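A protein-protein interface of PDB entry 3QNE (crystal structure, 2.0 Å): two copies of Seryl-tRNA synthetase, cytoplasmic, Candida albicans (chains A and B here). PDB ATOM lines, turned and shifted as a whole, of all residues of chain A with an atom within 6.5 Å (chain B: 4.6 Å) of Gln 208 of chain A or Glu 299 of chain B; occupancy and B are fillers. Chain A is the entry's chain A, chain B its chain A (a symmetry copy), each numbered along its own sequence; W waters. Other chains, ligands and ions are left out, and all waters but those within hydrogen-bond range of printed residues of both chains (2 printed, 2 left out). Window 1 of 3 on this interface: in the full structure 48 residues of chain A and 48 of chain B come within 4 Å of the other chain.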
ATOM      1  N   PRO A 206      -1.918  21.970   7.654  1.00  0.00           N
ATOM      2  CA  PRO A 206      -2.221  21.723   6.234  1.00  0.00           C
ATOM      3  C   PRO A 206      -3.495  22.454   5.824  1.00  0.00           C
ATOM      4  O   PRO A 206      -4.509  22.416   6.539  1.00  0.00           O
ATOM      5  CB  PRO A 206      -2.443  20.205   6.172  1.00  0.00           C
ATOM      6  CG  PRO A 206      -1.615  19.653   7.356  1.00  0.00           C
ATOM      7  CD  PRO A 206      -1.794  20.720   8.432  1.00  0.00           C
ATOM      8  N   LEU A 207      -3.440  23.121   4.682  1.00  0.00           N
ATOM      9  CA  LEU A 207      -4.585  23.896   4.217  1.00  0.00           C
ATOM     10  C   LEU A 207      -4.688  23.766   2.709  1.00  0.00           C
ATOM     11  O   LEU A 207      -3.802  24.207   2.001  1.00  0.00           O
ATOM     12  CB  LEU A 207      -4.400  25.356   4.604  1.00  0.00           C
ATOM     13  CG  LEU A 207      -5.632  26.258   4.612  1.00  0.00           C
ATOM     14  CD1 LEU A 207      -6.761  25.672   5.486  1.00  0.00           C
ATOM     15  CD2 LEU A 207      -5.216  27.624   5.101  1.00  0.00           C
ATOM     16  N   GLN A 208      -5.749  23.137   2.215  1.00  0.00           N
ATOM     17  CA  GLN A 208      -5.912  23.019   0.771  1.00  0.00           C
ATOM     18  C   GLN A 208      -6.873  24.087   0.329  1.00  0.00           C
ATOM     19  O   GLN A 208      -8.026  24.123   0.773  1.00  0.00           O
ATOM     20  CB  GLN A 208      -6.437  21.645   0.354  1.00  0.00           C
ATOM     21  CG  GLN A 208      -6.781  21.571  -1.140  1.00  0.00           C
ATOM     22  CD  GLN A 208      -7.081  20.156  -1.570  1.00  0.00           C
ATOM     23  OE1 GLN A 208      -6.644  19.208  -0.928  1.00  0.00           O
ATOM     24  NE2 GLN A 208      -7.824  20.005  -2.655  1.00  0.00           N
ATOM     25  N   ALA A 209      -6.382  24.977  -0.524  1.00  0.00           N
ATOM     26  CA  ALA A 209      -7.140  26.163  -0.906  1.00  0.00           C
ATOM     27  C   ALA A 209      -7.958  25.948  -2.176  1.00  0.00           C
ATOM     28  O   ALA A 209      -7.557  25.186  -3.048  1.00  0.00           O
ATOM     29  CB  ALA A 209      -6.180  27.370  -1.093  1.00  0.00           C
ATOM     30  N   PRO A 210      -9.092  26.645  -2.293  1.00  0.00           N
ATOM     31  CA  PRO A 210      -9.862  26.637  -3.543  1.00  0.00           C
ATOM     32  C   PRO A 210      -9.012  27.317  -4.584  1.00  0.00           C
ATOM     33  O   PRO A 210      -8.224  28.177  -4.201  1.00  0.00           O
ATOM     34  CB  PRO A 210     -11.086  27.510  -3.223  1.00  0.00           C
ATOM     35  CG  PRO A 210     -10.707  28.306  -2.044  1.00  0.00           C
ATOM     36  CD  PRO A 210      -9.713  27.492  -1.257  1.00  0.00           C
ATOM     37  N   SER A 247      -1.405  29.178  -3.948  1.00  0.00           N
ATOM     38  CA  SER A 247      -2.303  29.123  -2.799  1.00  0.00           C
ATOM     39  C   SER A 247      -2.048  30.302  -1.857  1.00  0.00           C
ATOM     40  O   SER A 247      -2.880  30.597  -0.997  1.00  0.00           O
ATOM     41  CB  SER A 247      -2.191  27.800  -2.023  1.00  0.00           C
ATOM     42  OG  SER A 247      -0.863  27.618  -1.552  1.00  0.00           O
ATOM     43  N   ILE A 251      -4.931  31.935   0.622  1.00  0.00           N
ATOM     44  CA  ILE A 251      -4.549  31.727   2.007  1.00  0.00           C
ATOM     45  C   ILE A 251      -4.221  33.066   2.680  1.00  0.00           C
ATOM     46  O   ILE A 251      -4.488  33.264   3.869  1.00  0.00           O
ATOM     47  CB  ILE A 251      -3.392  30.714   2.148  1.00  0.00           C
ATOM     48  CG1 ILE A 251      -3.880  29.302   1.733  1.00  0.00           C
ATOM     49  CG2 ILE A 251      -2.902  30.729   3.618  1.00  0.00           C
ATOM     50  CD1 ILE A 251      -2.770  28.202   1.740  1.00  0.00           C
ATOM     51  N   ALA A 272       0.701  25.166   5.797  1.00  0.00           N
ATOM     52  CA  ALA A 272       1.240  24.415   4.678  1.00  0.00           C
ATOM     53  C   ALA A 272       0.156  24.400   3.602  1.00  0.00           C
ATOM     54  O   ALA A 272      -0.744  23.537   3.595  1.00  0.00           O
ATOM     55  CB  ALA A 272       1.615  22.997   5.129  1.00  0.00           C
ATOM     56  N   GLY A 273       0.213  25.386   2.711  1.00  0.00           N
ATOM     57  CA  GLY A 273      -0.825  25.524   1.715  1.00  0.00           C
ATOM     58  C   GLY A 273      -0.594  24.547   0.568  1.00  0.00           C
ATOM     59  O   GLY A 273       0.541  24.296   0.181  1.00  0.00           O
ATOM     60  N   TYR A 274      -1.673  23.987   0.037  1.00  0.00           N
ATOM     61  CA  TYR A 274      -1.570  23.097  -1.122  1.00  0.00           C
ATOM     62  C   TYR A 274      -2.659  23.450  -2.112  1.00  0.00           C
ATOM     63  O   TYR A 274      -3.838  23.632  -1.728  1.00  0.00           O
ATOM     64  CB  TYR A 274      -1.700  21.619  -0.717  1.00  0.00           C
ATOM     65  CG  TYR A 274      -1.982  20.755  -1.926  1.00  0.00           C
ATOM     66  CD1 TYR A 274      -1.104  20.757  -3.027  1.00  0.00           C
ATOM     67  CD2 TYR A 274      -3.141  19.982  -2.009  1.00  0.00           C
ATOM     68  CE1 TYR A 274      -1.379  20.000  -4.161  1.00  0.00           C
ATOM     69  CE2 TYR A 274      -3.408  19.204  -3.143  1.00  0.00           C
ATOM     70  CZ  TYR A 274      -2.527  19.227  -4.215  1.00  0.00           C
ATOM     71  OH  TYR A 274      -2.789  18.480  -5.347  1.00  0.00           O
ATOM     72  N   SER A 275      -2.287  23.561  -3.386  1.00  0.00           N
ATOM     73  CA  SER A 275      -3.293  23.754  -4.420  1.00  0.00           C
ATOM     74  C   SER A 275      -2.635  23.580  -5.765  1.00  0.00           C
ATOM     75  O   SER A 275      -1.417  23.618  -5.875  1.00  0.00           O
ATOM     76  CB  SER A 275      -3.875  25.171  -4.359  1.00  0.00           C
ATOM     77  OG  SER A 275      -2.911  26.119  -4.832  1.00  0.00           O
ATOM     78  N   TYR B 178     -14.863  26.279  -0.156  1.00  0.00           N
ATOM     79  CA  TYR B 178     -14.326  25.658   1.053  1.00  0.00           C
ATOM     80  C   TYR B 178     -12.816  25.503   1.000  1.00  0.00           C
ATOM     81  O   TYR B 178     -12.230  25.352  -0.085  1.00  0.00           O
ATOM     82  CB  TYR B 178     -14.989  24.278   1.293  1.00  0.00           C
ATOM     83  CG  TYR B 178     -14.647  23.242   0.230  1.00  0.00           C
ATOM     84  CD1 TYR B 178     -13.632  22.325   0.432  1.00  0.00           C
ATOM     85  CD2 TYR B 178     -15.366  23.175  -0.975  1.00  0.00           C
ATOM     86  CE1 TYR B 178     -13.308  21.363  -0.545  1.00  0.00           C
ATOM     87  CE2 TYR B 178     -15.041  22.244  -1.962  1.00  0.00           C
ATOM     88  CZ  TYR B 178     -14.011  21.339  -1.741  1.00  0.00           C
ATOM     89  OH  TYR B 178     -13.685  20.410  -2.711  1.00  0.00           O
ATOM     90  N   PHE B 179     -12.185  25.558   2.168  1.00  0.00           N
ATOM     91  CA  PHE B 179     -10.825  25.034   2.299  1.00  0.00           C
ATOM     92  C   PHE B 179     -10.944  23.681   2.979  1.00  0.00           C
ATOM     93  O   PHE B 179     -11.852  23.485   3.781  1.00  0.00           O
ATOM     94  CB  PHE B 179     -10.011  25.906   3.243  1.00  0.00           C
ATOM     95  CG  PHE B 179      -9.677  27.272   2.704  1.00  0.00           C
ATOM     96  CD1 PHE B 179      -8.362  27.588   2.372  1.00  0.00           C
ATOM     97  CD2 PHE B 179     -10.665  28.250   2.571  1.00  0.00           C
ATOM     98  CE1 PHE B 179      -8.029  28.875   1.899  1.00  0.00           C
ATOM     99  CE2 PHE B 179     -10.352  29.536   2.100  1.00  0.00           C
ATOM    100  CZ  PHE B 179      -9.039  29.853   1.770  1.00  0.00           C
ATOM    101  N   LEU B 180     -10.012  22.772   2.711  1.00  0.00           N
ATOM    102  CA  LEU B 180      -9.842  21.589   3.564  1.00  0.00           C
ATOM    103  C   LEU B 180      -8.735  21.936   4.557  1.00  0.00           C
ATOM    104  O   LEU B 180      -7.849  22.708   4.235  1.00  0.00           O
ATOM    105  CB  LEU B 180      -9.438  20.360   2.729  1.00  0.00           C
ATOM    106  CG  LEU B 180     -10.519  19.886   1.754  1.00  0.00           C
ATOM    107  CD1 LEU B 180     -10.002  18.701   0.903  1.00  0.00           C
ATOM    108  CD2 LEU B 180     -11.814  19.477   2.510  1.00  0.00           C
ATOM    109  N   VAL B 185      -7.436  17.504   4.787  1.00  0.00           N
ATOM    110  CA  VAL B 185      -6.464  17.442   3.690  1.00  0.00           C
ATOM    111  C   VAL B 185      -5.887  16.024   3.608  1.00  0.00           C
ATOM    112  O   VAL B 185      -5.823  15.437   2.534  1.00  0.00           O
ATOM    113  CB  VAL B 185      -5.313  18.468   3.884  1.00  0.00           C
ATOM    114  CG1 VAL B 185      -4.232  18.318   2.772  1.00  0.00           C
ATOM    115  CG2 VAL B 185      -5.873  19.905   3.901  1.00  0.00           C
ATOM    116  N   ASN B 188      -8.321  13.500   2.172  1.00  0.00           N
ATOM    117  CA  ASN B 188      -8.506  13.656   0.735  1.00  0.00           C
ATOM    118  C   ASN B 188      -7.330  13.043  -0.023  1.00  0.00           C
ATOM    119  O   ASN B 188      -7.535  12.258  -0.949  1.00  0.00           O
ATOM    120  CB  ASN B 188      -8.675  15.117   0.345  1.00  0.00           C
ATOM    121  CG  ASN B 188      -9.384  15.272  -0.991  1.00  0.00           C
ATOM    122  OD1 ASN B 188     -10.468  14.707  -1.206  1.00  0.00           O
ATOM    123  ND2 ASN B 188      -8.791  16.053  -1.890  1.00  0.00           N
ATOM    124  N   ILE B 192      -7.099   9.802  -2.664  1.00  0.00           N
ATOM    125  CA  ILE B 192      -6.472   9.898  -3.978  1.00  0.00           C
ATOM    126  C   ILE B 192      -5.383   8.821  -4.145  1.00  0.00           C
ATOM    127  O   ILE B 192      -5.334   8.091  -5.142  1.00  0.00           O
ATOM    128  CB  ILE B 192      -5.860  11.308  -4.172  1.00  0.00           C
ATOM    129  CG1 ILE B 192      -6.969  12.367  -4.296  1.00  0.00           C
ATOM    130  CG2 ILE B 192      -4.967  11.336  -5.377  1.00  0.00           C
ATOM    131  CD1 ILE B 192      -6.466  13.787  -4.130  1.00  0.00           C
ATOM    132  N   TYR B 274      -6.818  10.842 -12.812  1.00  0.00           N
ATOM    133  CA  TYR B 274      -6.895  11.688 -11.619  1.00  0.00           C
ATOM    134  C   TYR B 274      -6.884  13.142 -12.046  1.00  0.00           C
ATOM    135  O   TYR B 274      -6.058  13.552 -12.894  1.00  0.00           O
ATOM    136  CB  TYR B 274      -5.725  11.424 -10.657  1.00  0.00           C
ATOM    137  CG  TYR B 274      -5.596  12.543  -9.649  1.00  0.00           C
ATOM    138  CD1 TYR B 274      -6.681  12.889  -8.820  1.00  0.00           C
ATOM    139  CD2 TYR B 274      -4.427  13.299  -9.553  1.00  0.00           C
ATOM    140  CE1 TYR B 274      -6.584  13.946  -7.921  1.00  0.00           C
ATOM    141  CE2 TYR B 274      -4.323  14.352  -8.634  1.00  0.00           C
ATOM    142  CZ  TYR B 274      -5.410  14.672  -7.831  1.00  0.00           C
ATOM    143  OH  TYR B 274      -5.327  15.720  -6.936  1.00  0.00           O
ATOM    144  N   SER B 275      -7.793  13.931 -11.478  1.00  0.00           N
ATOM    145  CA  SER B 275      -7.757  15.366 -11.720  1.00  0.00           C
ATOM    146  C   SER B 275      -8.711  16.036 -10.764  1.00  0.00           C
ATOM    147  O   SER B 275      -9.565  15.386 -10.175  1.00  0.00           O
ATOM    148  CB  SER B 275      -8.215  15.691 -13.147  1.00  0.00           C
ATOM    149  OG  SER B 275      -9.629  15.498 -13.266  1.00  0.00           O
ATOM    150  N   SER B 276      -8.570  17.343 -10.626  1.00  0.00           N
ATOM    151  CA  SER B 276      -9.657  18.125 -10.062  1.00  0.00           C
ATOM    152  C   SER B 276     -10.741  18.253 -11.138  1.00  0.00           C
ATOM    153  O   SER B 276     -10.471  18.038 -12.337  1.00  0.00           O
ATOM    154  CB  SER B 276      -9.159  19.485  -9.597  1.00  0.00           C
ATOM    155  OG  SER B 276      -8.358  19.305  -8.436  1.00  0.00           O
ATOM    156  N   PHE B 298     -13.799  19.725  -6.873  1.00  0.00           N
ATOM    157  CA  PHE B 298     -13.510  18.541  -6.079  1.00  0.00           C
ATOM    158  C   PHE B 298     -12.572  17.659  -6.899  1.00  0.00           C
ATOM    159  O   PHE B 298     -12.324  17.947  -8.084  1.00  0.00           O
ATOM    160  CB  PHE B 298     -14.814  17.785  -5.742  1.00  0.00           C
ATOM    161  CG  PHE B 298     -15.643  17.438  -6.958  1.00  0.00           C
ATOM    162  CD1 PHE B 298     -15.404  16.271  -7.671  1.00  0.00           C
ATOM    163  CD2 PHE B 298     -16.647  18.295  -7.400  1.00  0.00           C
ATOM    164  CE1 PHE B 298     -16.166  15.958  -8.801  1.00  0.00           C
ATOM    165  CE2 PHE B 298     -17.410  17.993  -8.523  1.00  0.00           C
ATOM    166  CZ  PHE B 298     -17.171  16.824  -9.229  1.00  0.00           C
ATOM    167  N   GLU B 299     -12.029  16.619  -6.272  1.00  0.00           N
ATOM    168  CA  GLU B 299     -11.115  15.688  -6.978  1.00  0.00           C
ATOM    169  C   GLU B 299     -11.809  14.357  -7.252  1.00  0.00           C
ATOM    170  O   GLU B 299     -12.735  13.958  -6.529  1.00  0.00           O
ATOM    171  CB  GLU B 299      -9.814  15.448  -6.194  1.00  0.00           C
ATOM    172  CG  GLU B 299      -8.869  16.646  -6.203  1.00  0.00           C
ATOM    173  CD  GLU B 299      -9.438  17.811  -5.401  1.00  0.00           C
ATOM    174  OE1 GLU B 299      -9.639  17.639  -4.183  1.00  0.00           O
ATOM    175  OE2 GLU B 299      -9.697  18.884  -5.978  1.00  0.00           O
ATOM    176  N   LYS B 300     -11.372  13.670  -8.309  1.00  0.00           N
ATOM    177  CA  LYS B 300     -11.963  12.379  -8.634  1.00  0.00           C
ATOM    178  C   LYS B 300     -10.899  11.436  -9.190  1.00  0.00           C
ATOM    179  O   LYS B 300     -10.062  11.859 -10.000  1.00  0.00           O
ATOM    180  CB  LYS B 300     -13.067  12.579  -9.684  1.00  0.00           C
ATOM    181  CG  LYS B 300     -13.822  11.324 -10.006  1.00  0.00           C
ATOM    182  CD  LYS B 300     -14.846  11.579 -11.099  1.00  0.00           C
ATOM    183  CE  LYS B 300     -15.850  12.615 -10.694  1.00  0.00           C
ATOM    184  NZ  LYS B 300     -17.006  12.614 -11.653  1.00  0.00           N
ATOM    185  N   ILE B 301     -10.928  10.188  -8.735  1.00  0.00           N
ATOM    186  CA  ILE B 301     -10.211   9.118  -9.407  1.00  0.00           C
ATOM    187  C   ILE B 301     -11.238   8.409 -10.267  1.00  0.00           C
ATOM    188  O   ILE B 301     -12.284   7.956  -9.770  1.00  0.00           O
ATOM    189  CB  ILE B 301      -9.582   8.091  -8.439  1.00  0.00           C
ATOM    190  CG1 ILE B 301      -8.640   8.753  -7.438  1.00  0.00           C
ATOM    191  CG2 ILE B 301      -8.796   7.031  -9.234  1.00  0.00           C
ATOM    192  CD1 ILE B 301      -7.501   9.456  -8.086  1.00  0.00           C
ATOM    193  N   SER B 406     -13.558   7.034  -7.146  1.00  0.00           N
ATOM    194  CA  SER B 406     -13.926   7.877  -6.011  1.00  0.00           C
ATOM    195  C   SER B 406     -13.944   9.371  -6.336  1.00  0.00           C
ATOM    196  O   SER B 406     -12.932   9.913  -6.717  1.00  0.00           O
ATOM    197  CB  SER B 406     -12.967   7.651  -4.841  1.00  0.00           C
ATOM    198  OG  SER B 406     -13.342   8.453  -3.719  1.00  0.00           O
ATOM    199  N   ALA B 407     -15.099  10.019  -6.186  1.00  0.00           N
ATOM    200  CA  ALA B 407     -15.137  11.469  -6.013  1.00  0.00           C
ATOM    201  C   ALA B 407     -14.723  11.717  -4.576  1.00  0.00           C
ATOM    202  O   ALA B 407     -15.482  11.413  -3.645  1.00  0.00           O
ATOM    203  CB  ALA B 407     -16.536  11.999  -6.270  1.00  0.00           C
ATOM    204  N   THR B 408     -13.501  12.205  -4.364  1.00  0.00           N
ATOM    205  CA  THR B 408     -12.897  11.990  -3.038  1.00  0.00           C
ATOM    206  C   THR B 408     -13.589  12.751  -1.884  1.00  0.00           C
ATOM    207  O   THR B 408     -13.817  12.195  -0.801  1.00  0.00           O
ATOM    208  CB  THR B 408     -11.377  12.236  -3.050  1.00  0.00           C
ATOM    209  OG1 THR B 408     -11.125  13.569  -3.500  1.00  0.00           O
ATOM    210  CG2 THR B 408     -10.668  11.224  -4.014  1.00  0.00           C
ATOM    211  N   GLU B 409     -13.916  14.015  -2.106  1.00  0.00           N
ATOM    212  CA  GLU B 409     -14.599  14.782  -1.056  1.00  0.00           C
ATOM    213  C   GLU B 409     -15.958  14.156  -0.742  1.00  0.00           C
ATOM    214  O   GLU B 409     -16.401  14.102   0.412  1.00  0.00           O
ATOM    215  CB  GLU B 409     -14.783  16.244  -1.468  1.00  0.00           C
ATOM    216  CG  GLU B 409     -13.490  17.100  -1.296  1.00  0.00           C
ATOM    217  CD  GLU B 409     -12.585  17.100  -2.535  1.00  0.00           C
ATOM    218  OE1 GLU B 409     -12.900  16.371  -3.497  1.00  0.00           O
ATOM    219  OE2 GLU B 409     -11.562  17.835  -2.542  1.00  0.00           O
HETATM  220  O   HOH W   1     -10.538  23.514  -1.109  1.00  0.00           O
HETATM  221  O   HOH W   2      -6.072  16.799  -1.366  1.00  0.00           O
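The side-chain amide nitrogen (NE2) of Gln 208 of chain A sits at hydrogen-bond distance from the side-chain carboxylate (OE1) of Glu 299 of chain B, 3.4 Å away. The backbone carbonyl oxygen of Leu 180 of chain B sits at hydrogen-bond distance from the backbone NH of Gln 208 of chain A.
The backbone NH (N) of Ala 209 of chain A is in hydrogen-bond range of the backbone carbonyl oxygen (O) of Tyr 274 of chain A (3.1 Å). The backbone carbonyl oxygen (O) of Glu 299 of chain B lies within hydrogen-bond range of the backbone NH (N) of Thr 408 of chain B (2.9 Å). The side-chain amide nitrogen (ND2) of Asn 188 of chain B sits at hydrogen-bond distance from the side-chain carboxylate (OE1) of Glu 299 of chain B (2.9 Å). OH of Tyr 178 of chain B lies within hydrogen-bond range of OE2 of Glu 409 of chain B. The backbone NH (N) of Tyr 274 of chain A lies within hydrogen-bond range of the backbone carbonyl oxygen (O) of Leu 207 of chain A (2.9 Å). The side-chain carboxylate (OE2) of Glu 299 of chain B is in hydrogen-bond range of the side-chain hydroxyl (OG) of Ser 276 of chain B.
O of Pro 206 of chain A touches CG2 of Val 185 of chain B (3.9 Å). CG of Leu 207 of chain A touches CD1 of Phe 179 of chain B, at 3.8 Å. O of Leu 180 of chain B touches CD1 of Leu 207 of chain A (3.4 Å). O of Gln 208 of chain A touches CA of Phe 179 of chain B, at 3.3 Å. Gln 208 of chain A touches Val 185 of chain B. Gln 208 of chain A touches Asn 188 of chain B. Ala 209 of chain A touches Phe 179 of chain B (CA to CD1, 3.8 Å). CD of Pro 210 of chain A touches O of Tyr 178 of chain B, at 3.5 Å. Pro 210 of chain A touches Phe 179 of chain B.
Of the printed residues of chain B, Leu 207 of chain A touches Phe 179 (3.8 Å) and Leu 180 (3.4 Å). Gln 208 of chain A touches five residues of chain B. Of the printed residues of chain A, Tyr 178 of chain B touches Pro 210 (3.5 Å). Of the printed residues of chain A, Phe 179 of chain B touches Leu 207 (3.8 Å), Gln 208 (3.3 Å), Ala 209 (3.8 Å) and Pro 210 (3.8 Å). Of the printed residues of chain A, Asn 188 of chain B touches Gln 208 (3.9 Å). Of chain A, only Gln 208 (3.4 Å) comes within 4 Å of Glu 299 of chain B. The nearest residue of chain B that does not touch Gln 208 of chain A is Glu 409 of chain B (4.3 Å). The nearest residue of chain A that does not touch Glu 299 of chain B is Tyr 274 of chain A (6.4 Å).
Of the 17 printed residues of chain B, 6 touch a printed residue of chain A. Of the 11 printed residues of chain A, 5 touch a printed residue of chain B. Hydrophobic or aromatic side chains of chain A within 4 Å of the printed part of chain B: Leu 207, Ala 209 and Pro 210. Among the printed residues, 11 pairs touch across the chains.
2 positions are printed for both chains.
Water W2 bridges OE1 of Gln 208 of chain A and ND2 of Asn 188 of chain B. Water W1 lies within hydrogen-bond range of the backbone carbonyl oxygen (O) of Tyr 178 of chain B (2.7 Å) and the backbone carbonyl oxygen (O) of Gln 208 of chain A (3.2 Å).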
